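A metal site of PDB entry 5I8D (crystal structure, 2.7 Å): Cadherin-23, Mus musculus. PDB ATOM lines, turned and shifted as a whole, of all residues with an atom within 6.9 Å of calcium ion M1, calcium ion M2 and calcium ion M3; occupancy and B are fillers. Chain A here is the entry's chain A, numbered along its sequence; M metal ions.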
ATOM      1  N   GLU A 133     -15.702  -2.174  10.904  1.00  0.00           N
ATOM      2  CA  GLU A 133     -16.184  -2.319  12.276  1.00  0.00           C
ATOM      3  C   GLU A 133     -15.357  -3.297  13.143  1.00  0.00           C
ATOM      4  O   GLU A 133     -14.672  -4.171  12.613  1.00  0.00           O
ATOM      5  CB  GLU A 133     -17.660  -2.758  12.151  1.00  0.00           C
ATOM      6  CG  GLU A 133     -18.366  -3.220  13.401  1.00  0.00           C
ATOM      7  CD  GLU A 133     -19.794  -3.670  13.109  1.00  0.00           C
ATOM      8  OE1 GLU A 133     -20.486  -3.956  14.114  1.00  0.00           O
ATOM      9  OE2 GLU A 133     -20.209  -3.767  11.909  1.00  0.00           O
ATOM     10  N   ASN A 134     -15.424  -3.131  14.484  1.00  0.00           N
ATOM     11  CA  ASN A 134     -14.675  -4.020  15.443  1.00  0.00           C
ATOM     12  C   ASN A 134     -13.165  -4.101  15.199  1.00  0.00           C
ATOM     13  O   ASN A 134     -12.609  -5.161  14.982  1.00  0.00           O
ATOM     14  CB  ASN A 134     -15.202  -5.467  15.427  1.00  0.00           C
ATOM     15  CG  ASN A 134     -16.654  -5.556  15.751  1.00  0.00           C
ATOM     16  OD1 ASN A 134     -17.105  -4.992  16.729  1.00  0.00           O
ATOM     17  ND2 ASN A 134     -17.402  -6.282  14.934  1.00  0.00           N
ATOM     18  N   ILE A 185     -15.624   0.218  18.210  1.00  0.00           N
ATOM     19  CA  ILE A 185     -16.146   0.821  16.964  1.00  0.00           C
ATOM     20  C   ILE A 185     -17.216  -0.080  16.382  1.00  0.00           C
ATOM     21  O   ILE A 185     -16.912  -1.050  15.644  1.00  0.00           O
ATOM     22  CB  ILE A 185     -15.024   1.035  15.923  1.00  0.00           C
ATOM     23  CG1 ILE A 185     -13.967   2.001  16.460  1.00  0.00           C
ATOM     24  CG2 ILE A 185     -15.574   1.510  14.572  1.00  0.00           C
ATOM     25  CD1 ILE A 185     -14.478   3.372  16.862  1.00  0.00           C
ATOM     26  N   ASP A 186     -18.462   0.250  16.725  1.00  0.00           N
ATOM     27  CA  ASP A 186     -19.663  -0.491  16.316  1.00  0.00           C
ATOM     28  C   ASP A 186     -20.515   0.277  15.306  1.00  0.00           C
ATOM     29  O   ASP A 186     -21.188   1.262  15.655  1.00  0.00           O
ATOM     30  CB  ASP A 186     -20.509  -0.806  17.546  1.00  0.00           C
ATOM     31  CG  ASP A 186     -21.685  -1.728  17.244  1.00  0.00           C
ATOM     32  OD1 ASP A 186     -21.721  -2.330  16.154  1.00  0.00           O
ATOM     33  OD2 ASP A 186     -22.576  -1.858  18.103  1.00  0.00           O
ATOM     34  N   ARG A 187     -20.517  -0.200  14.070  1.00  0.00           N
ATOM     35  CA  ARG A 187     -21.380   0.351  13.008  1.00  0.00           C
ATOM     36  C   ARG A 187     -22.865   0.423  13.364  1.00  0.00           C
ATOM     37  O   ARG A 187     -23.588   1.271  12.808  1.00  0.00           O
ATOM     38  CB  ARG A 187     -21.248  -0.459  11.724  1.00  0.00           C
ATOM     39  CG  ARG A 187     -21.590   0.359  10.486  1.00  0.00           C
ATOM     40  CD  ARG A 187     -22.005  -0.513   9.334  1.00  0.00           C
ATOM     41  NE  ARG A 187     -23.289  -1.157   9.612  1.00  0.00           N
ATOM     42  CZ  ARG A 187     -24.500  -0.642   9.391  1.00  0.00           C
ATOM     43  NH1 ARG A 187     -24.663   0.583   8.844  1.00  0.00           N
ATOM     44  NH2 ARG A 187     -25.563  -1.362   9.714  1.00  0.00           N
ATOM     45  N   GLU A 188     -23.319  -0.465  14.246  1.00  0.00           N
ATOM     46  CA  GLU A 188     -24.702  -0.447  14.748  1.00  0.00           C
ATOM     47  C   GLU A 188     -24.948   0.669  15.777  1.00  0.00           C
ATOM     48  O   GLU A 188     -26.085   1.092  15.958  1.00  0.00           O
ATOM     49  CB  GLU A 188     -25.127  -1.823  15.304  1.00  0.00           C
ATOM     50  CG  GLU A 188     -25.504  -2.855  14.242  1.00  0.00           C
ATOM     51  CD  GLU A 188     -24.376  -3.205  13.270  1.00  0.00           C
ATOM     52  OE1 GLU A 188     -24.501  -2.921  12.043  1.00  0.00           O
ATOM     53  OE2 GLU A 188     -23.349  -3.796  13.728  1.00  0.00           O
ATOM     54  N   GLU A 189     -23.881   1.122  16.439  1.00  0.00           N
ATOM     55  CA  GLU A 189     -23.918   2.306  17.333  1.00  0.00           C
ATOM     56  C   GLU A 189     -23.734   3.576  16.512  1.00  0.00           C
ATOM     57  O   GLU A 189     -24.487   4.522  16.688  1.00  0.00           O
ATOM     58  CB  GLU A 189     -22.856   2.228  18.449  1.00  0.00           C
ATOM     59  CG  GLU A 189     -22.707   3.496  19.279  1.00  0.00           C
ATOM     60  CD  GLU A 189     -22.034   3.232  20.621  1.00  0.00           C
ATOM     61  OE1 GLU A 189     -22.639   3.599  21.656  1.00  0.00           O
ATOM     62  OE2 GLU A 189     -20.914   2.682  20.639  1.00  0.00           O
ATOM     63  N   ASP A 218     -17.600   0.550   7.856  1.00  0.00           N
ATOM     64  CA  ASP A 218     -18.057  -0.583   7.029  1.00  0.00           C
ATOM     65  C   ASP A 218     -18.613  -1.680   7.931  1.00  0.00           C
ATOM     66  O   ASP A 218     -18.290  -1.747   9.117  1.00  0.00           O
ATOM     67  CB  ASP A 218     -16.951  -1.084   6.091  1.00  0.00           C
ATOM     68  CG  ASP A 218     -16.793  -0.215   4.835  1.00  0.00           C
ATOM     69  OD1 ASP A 218     -17.461   0.846   4.749  1.00  0.00           O
ATOM     70  OD2 ASP A 218     -16.005  -0.576   3.940  1.00  0.00           O
ATOM     71  N   ASP A 219     -19.473  -2.516   7.365  1.00  0.00           N
ATOM     72  CA  ASP A 219     -20.261  -3.480   8.126  1.00  0.00           C
ATOM     73  C   ASP A 219     -19.653  -4.865   8.096  1.00  0.00           C
ATOM     74  O   ASP A 219     -19.323  -5.378   7.030  1.00  0.00           O
ATOM     75  CB  ASP A 219     -21.670  -3.578   7.545  1.00  0.00           C
ATOM     76  CG  ASP A 219     -22.551  -4.536   8.318  1.00  0.00           C
ATOM     77  OD1 ASP A 219     -22.702  -4.329   9.544  1.00  0.00           O
ATOM     78  OD2 ASP A 219     -23.080  -5.478   7.703  1.00  0.00           O
ATOM     79  N   ILE A 220     -19.529  -5.469   9.282  1.00  0.00           N
ATOM     80  CA  ILE A 220     -19.483  -6.903   9.415  1.00  0.00           C
ATOM     81  C   ILE A 220     -20.891  -7.247   9.901  1.00  0.00           C
ATOM     82  O   ILE A 220     -21.454  -6.526  10.721  1.00  0.00           O
ATOM     83  CB  ILE A 220     -18.451  -7.346  10.483  1.00  0.00           C
ATOM     84  CG1 ILE A 220     -17.028  -6.968  10.062  1.00  0.00           C
ATOM     85  CG2 ILE A 220     -18.512  -8.860  10.708  1.00  0.00           C
ATOM     86  CD1 ILE A 220     -16.022  -6.976  11.209  1.00  0.00           C
ATOM     87  N   ASN A 221     -21.467  -8.336   9.379  1.00  0.00           N
ATOM     88  CA  ASN A 221     -22.755  -8.854   9.891  1.00  0.00           C
ATOM     89  C   ASN A 221     -22.545  -9.596  11.224  1.00  0.00           C
ATOM     90  O   ASN A 221     -22.340 -10.828  11.250  1.00  0.00           O
ATOM     91  CB  ASN A 221     -23.435  -9.747   8.853  1.00  0.00           C
ATOM     92  CG  ASN A 221     -24.865 -10.093   9.256  1.00  0.00           C
ATOM     93  OD1 ASN A 221     -25.141 -10.490  10.392  1.00  0.00           O
ATOM     94  ND2 ASN A 221     -25.798  -9.939   8.311  1.00  0.00           N
ATOM     95  N   ASP A 222     -22.634  -8.837  12.316  1.00  0.00           N
ATOM     96  CA  ASP A 222     -22.233  -9.319  13.622  1.00  0.00           C
ATOM     97  C   ASP A 222     -23.228  -9.050  14.741  1.00  0.00           C
ATOM     98  O   ASP A 222     -22.889  -9.204  15.910  1.00  0.00           O
ATOM     99  CB  ASP A 222     -20.905  -8.659  13.985  1.00  0.00           C
ATOM    100  CG  ASP A 222     -21.034  -7.183  14.252  1.00  0.00           C
ATOM    101  OD1 ASP A 222     -22.027  -6.543  13.822  1.00  0.00           O
ATOM    102  OD2 ASP A 222     -20.125  -6.645  14.906  1.00  0.00           O
ATOM    103  N   SER A 223     -24.453  -8.677  14.394  1.00  0.00           N
ATOM    104  CA  SER A 223     -25.448  -8.269  15.364  1.00  0.00           C
ATOM    105  C   SER A 223     -26.589  -9.281  15.309  1.00  0.00           C
ATOM    106  O   SER A 223     -27.101  -9.573  14.192  1.00  0.00           O
ATOM    107  CB  SER A 223     -25.961  -6.892  14.999  1.00  0.00           C
ATOM    108  OG  SER A 223     -26.606  -6.310  16.101  1.00  0.00           O
ATOM    109  N   ARG A 224     -26.961  -9.859  16.460  1.00  0.00           N
ATOM    110  CA  ARG A 224     -27.985 -10.925  16.461  1.00  0.00           C
ATOM    111  C   ARG A 224     -29.391 -10.376  16.224  1.00  0.00           C
ATOM    112  O   ARG A 224     -29.711  -9.263  16.661  1.00  0.00           O
ATOM    113  CB  ARG A 224     -27.924 -11.810  17.737  1.00  0.00           C
ATOM    114  CG  ARG A 224     -28.360 -11.132  19.029  1.00  0.00           C
ATOM    115  CD  ARG A 224     -28.508 -12.114  20.194  1.00  0.00           C
ATOM    116  NE  ARG A 224     -27.223 -12.475  20.800  1.00  0.00           N
ATOM    117  CZ  ARG A 224     -26.509 -13.570  20.525  1.00  0.00           C
ATOM    118  NH1 ARG A 224     -26.922 -14.447  19.605  1.00  0.00           N
ATOM    119  NH2 ARG A 224     -25.361 -13.783  21.172  1.00  0.00           N
ATOM    120  N   PRO A 225     -30.251 -11.148  15.533  1.00  0.00           N
ATOM    121  CA  PRO A 225     -31.610 -10.728  15.349  1.00  0.00           C
ATOM    122  C   PRO A 225     -32.353 -10.738  16.668  1.00  0.00           C
ATOM    123  O   PRO A 225     -32.159 -11.640  17.510  1.00  0.00           O
ATOM    124  CB  PRO A 225     -32.185 -11.769  14.388  1.00  0.00           C
ATOM    125  CG  PRO A 225     -31.352 -12.960  14.559  1.00  0.00           C
ATOM    126  CD  PRO A 225     -29.987 -12.445  14.882  1.00  0.00           C
ATOM    127  N   ASP A 253     -33.098  -7.041  12.633  1.00  0.00           N
ATOM    128  CA  ASP A 253     -31.659  -7.264  12.611  1.00  0.00           C
ATOM    129  C   ASP A 253     -31.045  -5.975  12.106  1.00  0.00           C
ATOM    130  O   ASP A 253     -31.377  -5.535  11.015  1.00  0.00           O
ATOM    131  CB  ASP A 253     -31.313  -8.422  11.689  1.00  0.00           C
ATOM    132  CG  ASP A 253     -29.957  -9.057  11.994  1.00  0.00           C
ATOM    133  OD1 ASP A 253     -28.900  -8.548  11.570  1.00  0.00           O
ATOM    134  OD2 ASP A 253     -29.920 -10.129  12.644  1.00  0.00           O
ATOM    135  N   LEU A 254     -30.159  -5.384  12.894  1.00  0.00           N
ATOM    136  CA  LEU A 254     -29.632  -4.052  12.586  1.00  0.00           C
ATOM    137  C   LEU A 254     -28.429  -4.028  11.646  1.00  0.00           C
ATOM    138  O   LEU A 254     -27.892  -2.959  11.355  1.00  0.00           O
ATOM    139  CB  LEU A 254     -29.277  -3.336  13.879  1.00  0.00           C
ATOM    140  CG  LEU A 254     -30.427  -3.187  14.870  1.00  0.00           C
ATOM    141  CD1 LEU A 254     -29.889  -2.759  16.224  1.00  0.00           C
ATOM    142  CD2 LEU A 254     -31.447  -2.207  14.348  1.00  0.00           C
ATOM    143  N   ASP A 255     -28.012  -5.194  11.154  1.00  0.00           N
ATOM    144  CA  ASP A 255     -26.937  -5.274  10.161  1.00  0.00           C
ATOM    145  C   ASP A 255     -27.427  -4.842   8.781  1.00  0.00           C
ATOM    146  O   ASP A 255     -28.617  -4.569   8.580  1.00  0.00           O
ATOM    147  CB  ASP A 255     -26.351  -6.699  10.135  1.00  0.00           C
ATOM    148  CG  ASP A 255     -25.479  -7.001  11.342  1.00  0.00           C
ATOM    149  OD1 ASP A 255     -24.559  -6.201  11.618  1.00  0.00           O
ATOM    150  OD2 ASP A 255     -25.698  -8.048  12.010  1.00  0.00           O
ATOM    151  N   LEU A 256     -26.500  -4.795   7.837  1.00  0.00           N
ATOM    152  CA  LEU A 256     -26.711  -4.165   6.544  1.00  0.00           C
ATOM    153  C   LEU A 256     -27.576  -4.971   5.576  1.00  0.00           C
ATOM    154  O   LEU A 256     -28.377  -4.396   4.866  1.00  0.00           O
ATOM    155  CB  LEU A 256     -25.356  -3.819   5.921  1.00  0.00           C
ATOM    156  CG  LEU A 256     -25.259  -2.607   4.975  1.00  0.00           C
ATOM    157  CD1 LEU A 256     -25.794  -1.318   5.578  1.00  0.00           C
ATOM    158  CD2 LEU A 256     -23.801  -2.438   4.568  1.00  0.00           C
ATOM    159  N   PRO A 258     -29.392  -8.451   6.162  1.00  0.00           N
ATOM    160  CA  PRO A 258     -29.757  -9.665   6.860  1.00  0.00           C
ATOM    161  C   PRO A 258     -30.692 -10.550   6.060  1.00  0.00           C
ATOM    162  O   PRO A 258     -31.556 -10.045   5.357  1.00  0.00           O
ATOM    163  CB  PRO A 258     -30.458  -9.164   8.120  1.00  0.00           C
ATOM    164  CG  PRO A 258     -30.947  -7.808   7.786  1.00  0.00           C
ATOM    165  CD  PRO A 258     -30.145  -7.280   6.642  1.00  0.00           C
ATOM    166  N   LEU A 260     -33.057 -13.149   7.371  1.00  0.00           N
ATOM    167  CA  LEU A 260     -33.720 -13.751   8.511  1.00  0.00           C
ATOM    168  C   LEU A 260     -34.622 -14.917   8.122  1.00  0.00           C
ATOM    169  O   LEU A 260     -35.499 -14.762   7.284  1.00  0.00           O
ATOM    170  CB  LEU A 260     -34.585 -12.701   9.222  1.00  0.00           C
ATOM    171  CG  LEU A 260     -33.943 -11.404   9.719  1.00  0.00           C
ATOM    172  CD1 LEU A 260     -34.742 -10.848  10.884  1.00  0.00           C
ATOM    173  CD2 LEU A 260     -32.523 -11.591  10.173  1.00  0.00           C
ATOM    174  N   ASP A 315     -30.118 -15.357  11.276  1.00  0.00           N
ATOM    175  CA  ASP A 315     -29.611 -14.501  10.205  1.00  0.00           C
ATOM    176  C   ASP A 315     -28.625 -15.273   9.290  1.00  0.00           C
ATOM    177  O   ASP A 315     -27.431 -15.359   9.560  1.00  0.00           O
ATOM    178  CB  ASP A 315     -28.946 -13.264  10.820  1.00  0.00           C
ATOM    179  CG  ASP A 315     -28.632 -12.165   9.803  1.00  0.00           C
ATOM    180  OD1 ASP A 315     -28.837 -12.381   8.592  1.00  0.00           O
ATOM    181  OD2 ASP A 315     -28.186 -11.068  10.242  1.00  0.00           O
ATOM    182  N   ALA A 317     -27.171 -14.562   6.633  1.00  0.00           N
ATOM    183  CA  ALA A 317     -26.045 -13.745   6.194  1.00  0.00           C
ATOM    184  C   ALA A 317     -24.982 -13.537   7.266  1.00  0.00           C
ATOM    185  O   ALA A 317     -23.946 -12.960   6.977  1.00  0.00           O
ATOM    186  CB  ALA A 317     -26.565 -12.383   5.716  1.00  0.00           C
ATOM    187  N   SER A 318     -25.220 -14.008   8.490  1.00  0.00           N
ATOM    188  CA  SER A 318     -24.319 -13.746   9.632  1.00  0.00           C
ATOM    189  C   SER A 318     -22.852 -14.117   9.408  1.00  0.00           C
ATOM    190  O   SER A 318     -22.557 -15.198   8.911  1.00  0.00           O
ATOM    191  CB  SER A 318     -24.814 -14.500  10.865  1.00  0.00           C
ATOM    192  OG  SER A 318     -23.854 -14.379  11.959  1.00  0.00           O
ATOM    193  N   ASP A 319     -21.945 -13.206   9.814  1.00  0.00           N
ATOM    194  CA  ASP A 319     -20.488 -13.451   9.701  1.00  0.00           C
ATOM    195  C   ASP A 319     -19.877 -14.064  10.975  1.00  0.00           C
ATOM    196  O   ASP A 319     -18.726 -14.507  10.945  1.00  0.00           O
ATOM    197  CB  ASP A 319     -19.762 -12.159   9.328  1.00  0.00           C
ATOM    198  CG  ASP A 319     -20.041 -11.697   7.891  1.00  0.00           C
ATOM    199  OD1 ASP A 319     -19.831 -12.484   6.940  1.00  0.00           O
ATOM    200  OD2 ASP A 319     -20.438 -10.525   7.710  1.00  0.00           O
ATOM    201  N   HIS A 323     -23.461 -14.631  16.838  1.00  0.00           N
ATOM    202  CA  HIS A 323     -24.448 -13.552  16.732  1.00  0.00           C
ATOM    203  C   HIS A 323     -25.386 -13.766  15.530  1.00  0.00           C
ATOM    204  O   HIS A 323     -25.716 -12.815  14.770  1.00  0.00           O
ATOM    205  CB  HIS A 323     -23.736 -12.192  16.677  1.00  0.00           C
ATOM    206  CG  HIS A 323     -22.913 -11.889  17.896  1.00  0.00           C
ATOM    207  ND1 HIS A 323     -21.883 -10.966  17.881  1.00  0.00           N
ATOM    208  CD2 HIS A 323     -22.962 -12.373  19.157  1.00  0.00           C
ATOM    209  CE1 HIS A 323     -21.340 -10.913  19.090  1.00  0.00           C
ATOM    210  NE2 HIS A 323     -21.978 -11.746  19.877  1.00  0.00           N
ATOM    211  N   SER A 324     -25.810 -15.025  15.351  1.00  0.00           N
ATOM    212  CA  SER A 324     -26.653 -15.442  14.220  1.00  0.00           C
ATOM    213  C   SER A 324     -28.056 -15.842  14.621  1.00  0.00           C
ATOM    214  O   SER A 324     -28.948 -15.772  13.793  1.00  0.00           O
ATOM    215  CB  SER A 324     -25.992 -16.612  13.468  1.00  0.00           C
ATOM    216  OG  SER A 324     -25.601 -17.656  14.337  1.00  0.00           O
HETATM  217 CA    CA M   1     -27.183 -10.121  12.014  1.00  0.00          CA
HETATM  218 CA    CA M   2     -22.572  -4.854  11.778  1.00  0.00          CA
HETATM  219 CA    CA M   3     -21.719  -4.515  15.445  1.00  0.00          CA
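The backbone carbonyl oxygen of Asp 218 lies within hydrogen-bond range of the backbone NH of Glu 133, 3.2 Å away. N of Asp 315 is in hydrogen-bond range of O of Ser 324 (2.8 Å). The side-chain carboxylate (OD1) of Asp 315 lies close to the backbone NH (N) of Ala 317 (3.4 Å). The side-chain carboxylate (OD2) of Asp 219 sits close to the backbone NH (N) of Leu 256 (3.5 Å). NH2 of Arg 187 sits close to OE1 of Glu 188, 3.0 Å away. A ring nitrogen (ND1) of His 323 is in hydrogen-bond range of the backbone carbonyl oxygen (O) of Asp 222 (2.8 Å). OD2 of Asp 222 lies close to ND2 of Asn 134, at 2.7 Å. The backbone carbonyl oxygen (O) of Asn 221 is in hydrogen-bond range of the backbone NH (N) of Asp 319 (2.8 Å).
Of the 27 residues printed, 6 come within 4 Å of calcium ion M2. The nearest printed residue that does not touch calcium ion M2 is Arg 187 (4.3 Å).
Four residues have an atom within 4 Å of calcium ion M3: Glu 133, Asp 186, Glu 188 and Asp 222. The nearest printed residue that does not touch calcium ion M3 is Arg 187 (4.7 Å).
Calcium ion M1 is bound by the side-chain carboxylate (OD2) of Asp 315 (2.2 Å), the backbone carbonyl oxygen (O) of Ser 223 (2.2 Å), the side-chain carboxylate (OD1) of Asp 253 (2.4 Å), the side-chain carboxylate (OD2) of Asp 255 (2.6 Å), the side-chain amide oxygen (OD1) of Asn 221 (2.6 Å) and the side-chain carboxylate (OD2) of Asp 253 (2.8 Å).
Calcium ion M2 is bound by the backbone carbonyl oxygen (O) of Ile 220, 2.3 Å away. Calcium ion M2 is bound by the side-chain carboxylate (OD1) of Asp 219 (2.3 Å). Calcium ion M2 is bound by OE2 of Glu 188, 2.4 Å away. OD1 of Asp 255 is bound to calcium ion M2 (2.4 Å). Calcium ion M2 is bound by OE2 of Glu 133, 2.6 Å away. OD1 of Asp 222 binds calcium ion M2, 2.7 Å away. Calcium ion M2 is bound by the side-chain carboxylate (OE1) of Glu 188, at 2.7 Å. Calcium ion M2 has seven donor atoms within binding distance.
Calcium ion M3 is bound by the side-chain carboxylate (OE1) of Glu 133, the side-chain carboxylate (OD1) of Asp 186, the side-chain carboxylate (OE2) of Glu 188, the side-chain carboxylate (OD1) of Asp 222 and the side-chain carboxylate (OD2) of Asp 222.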
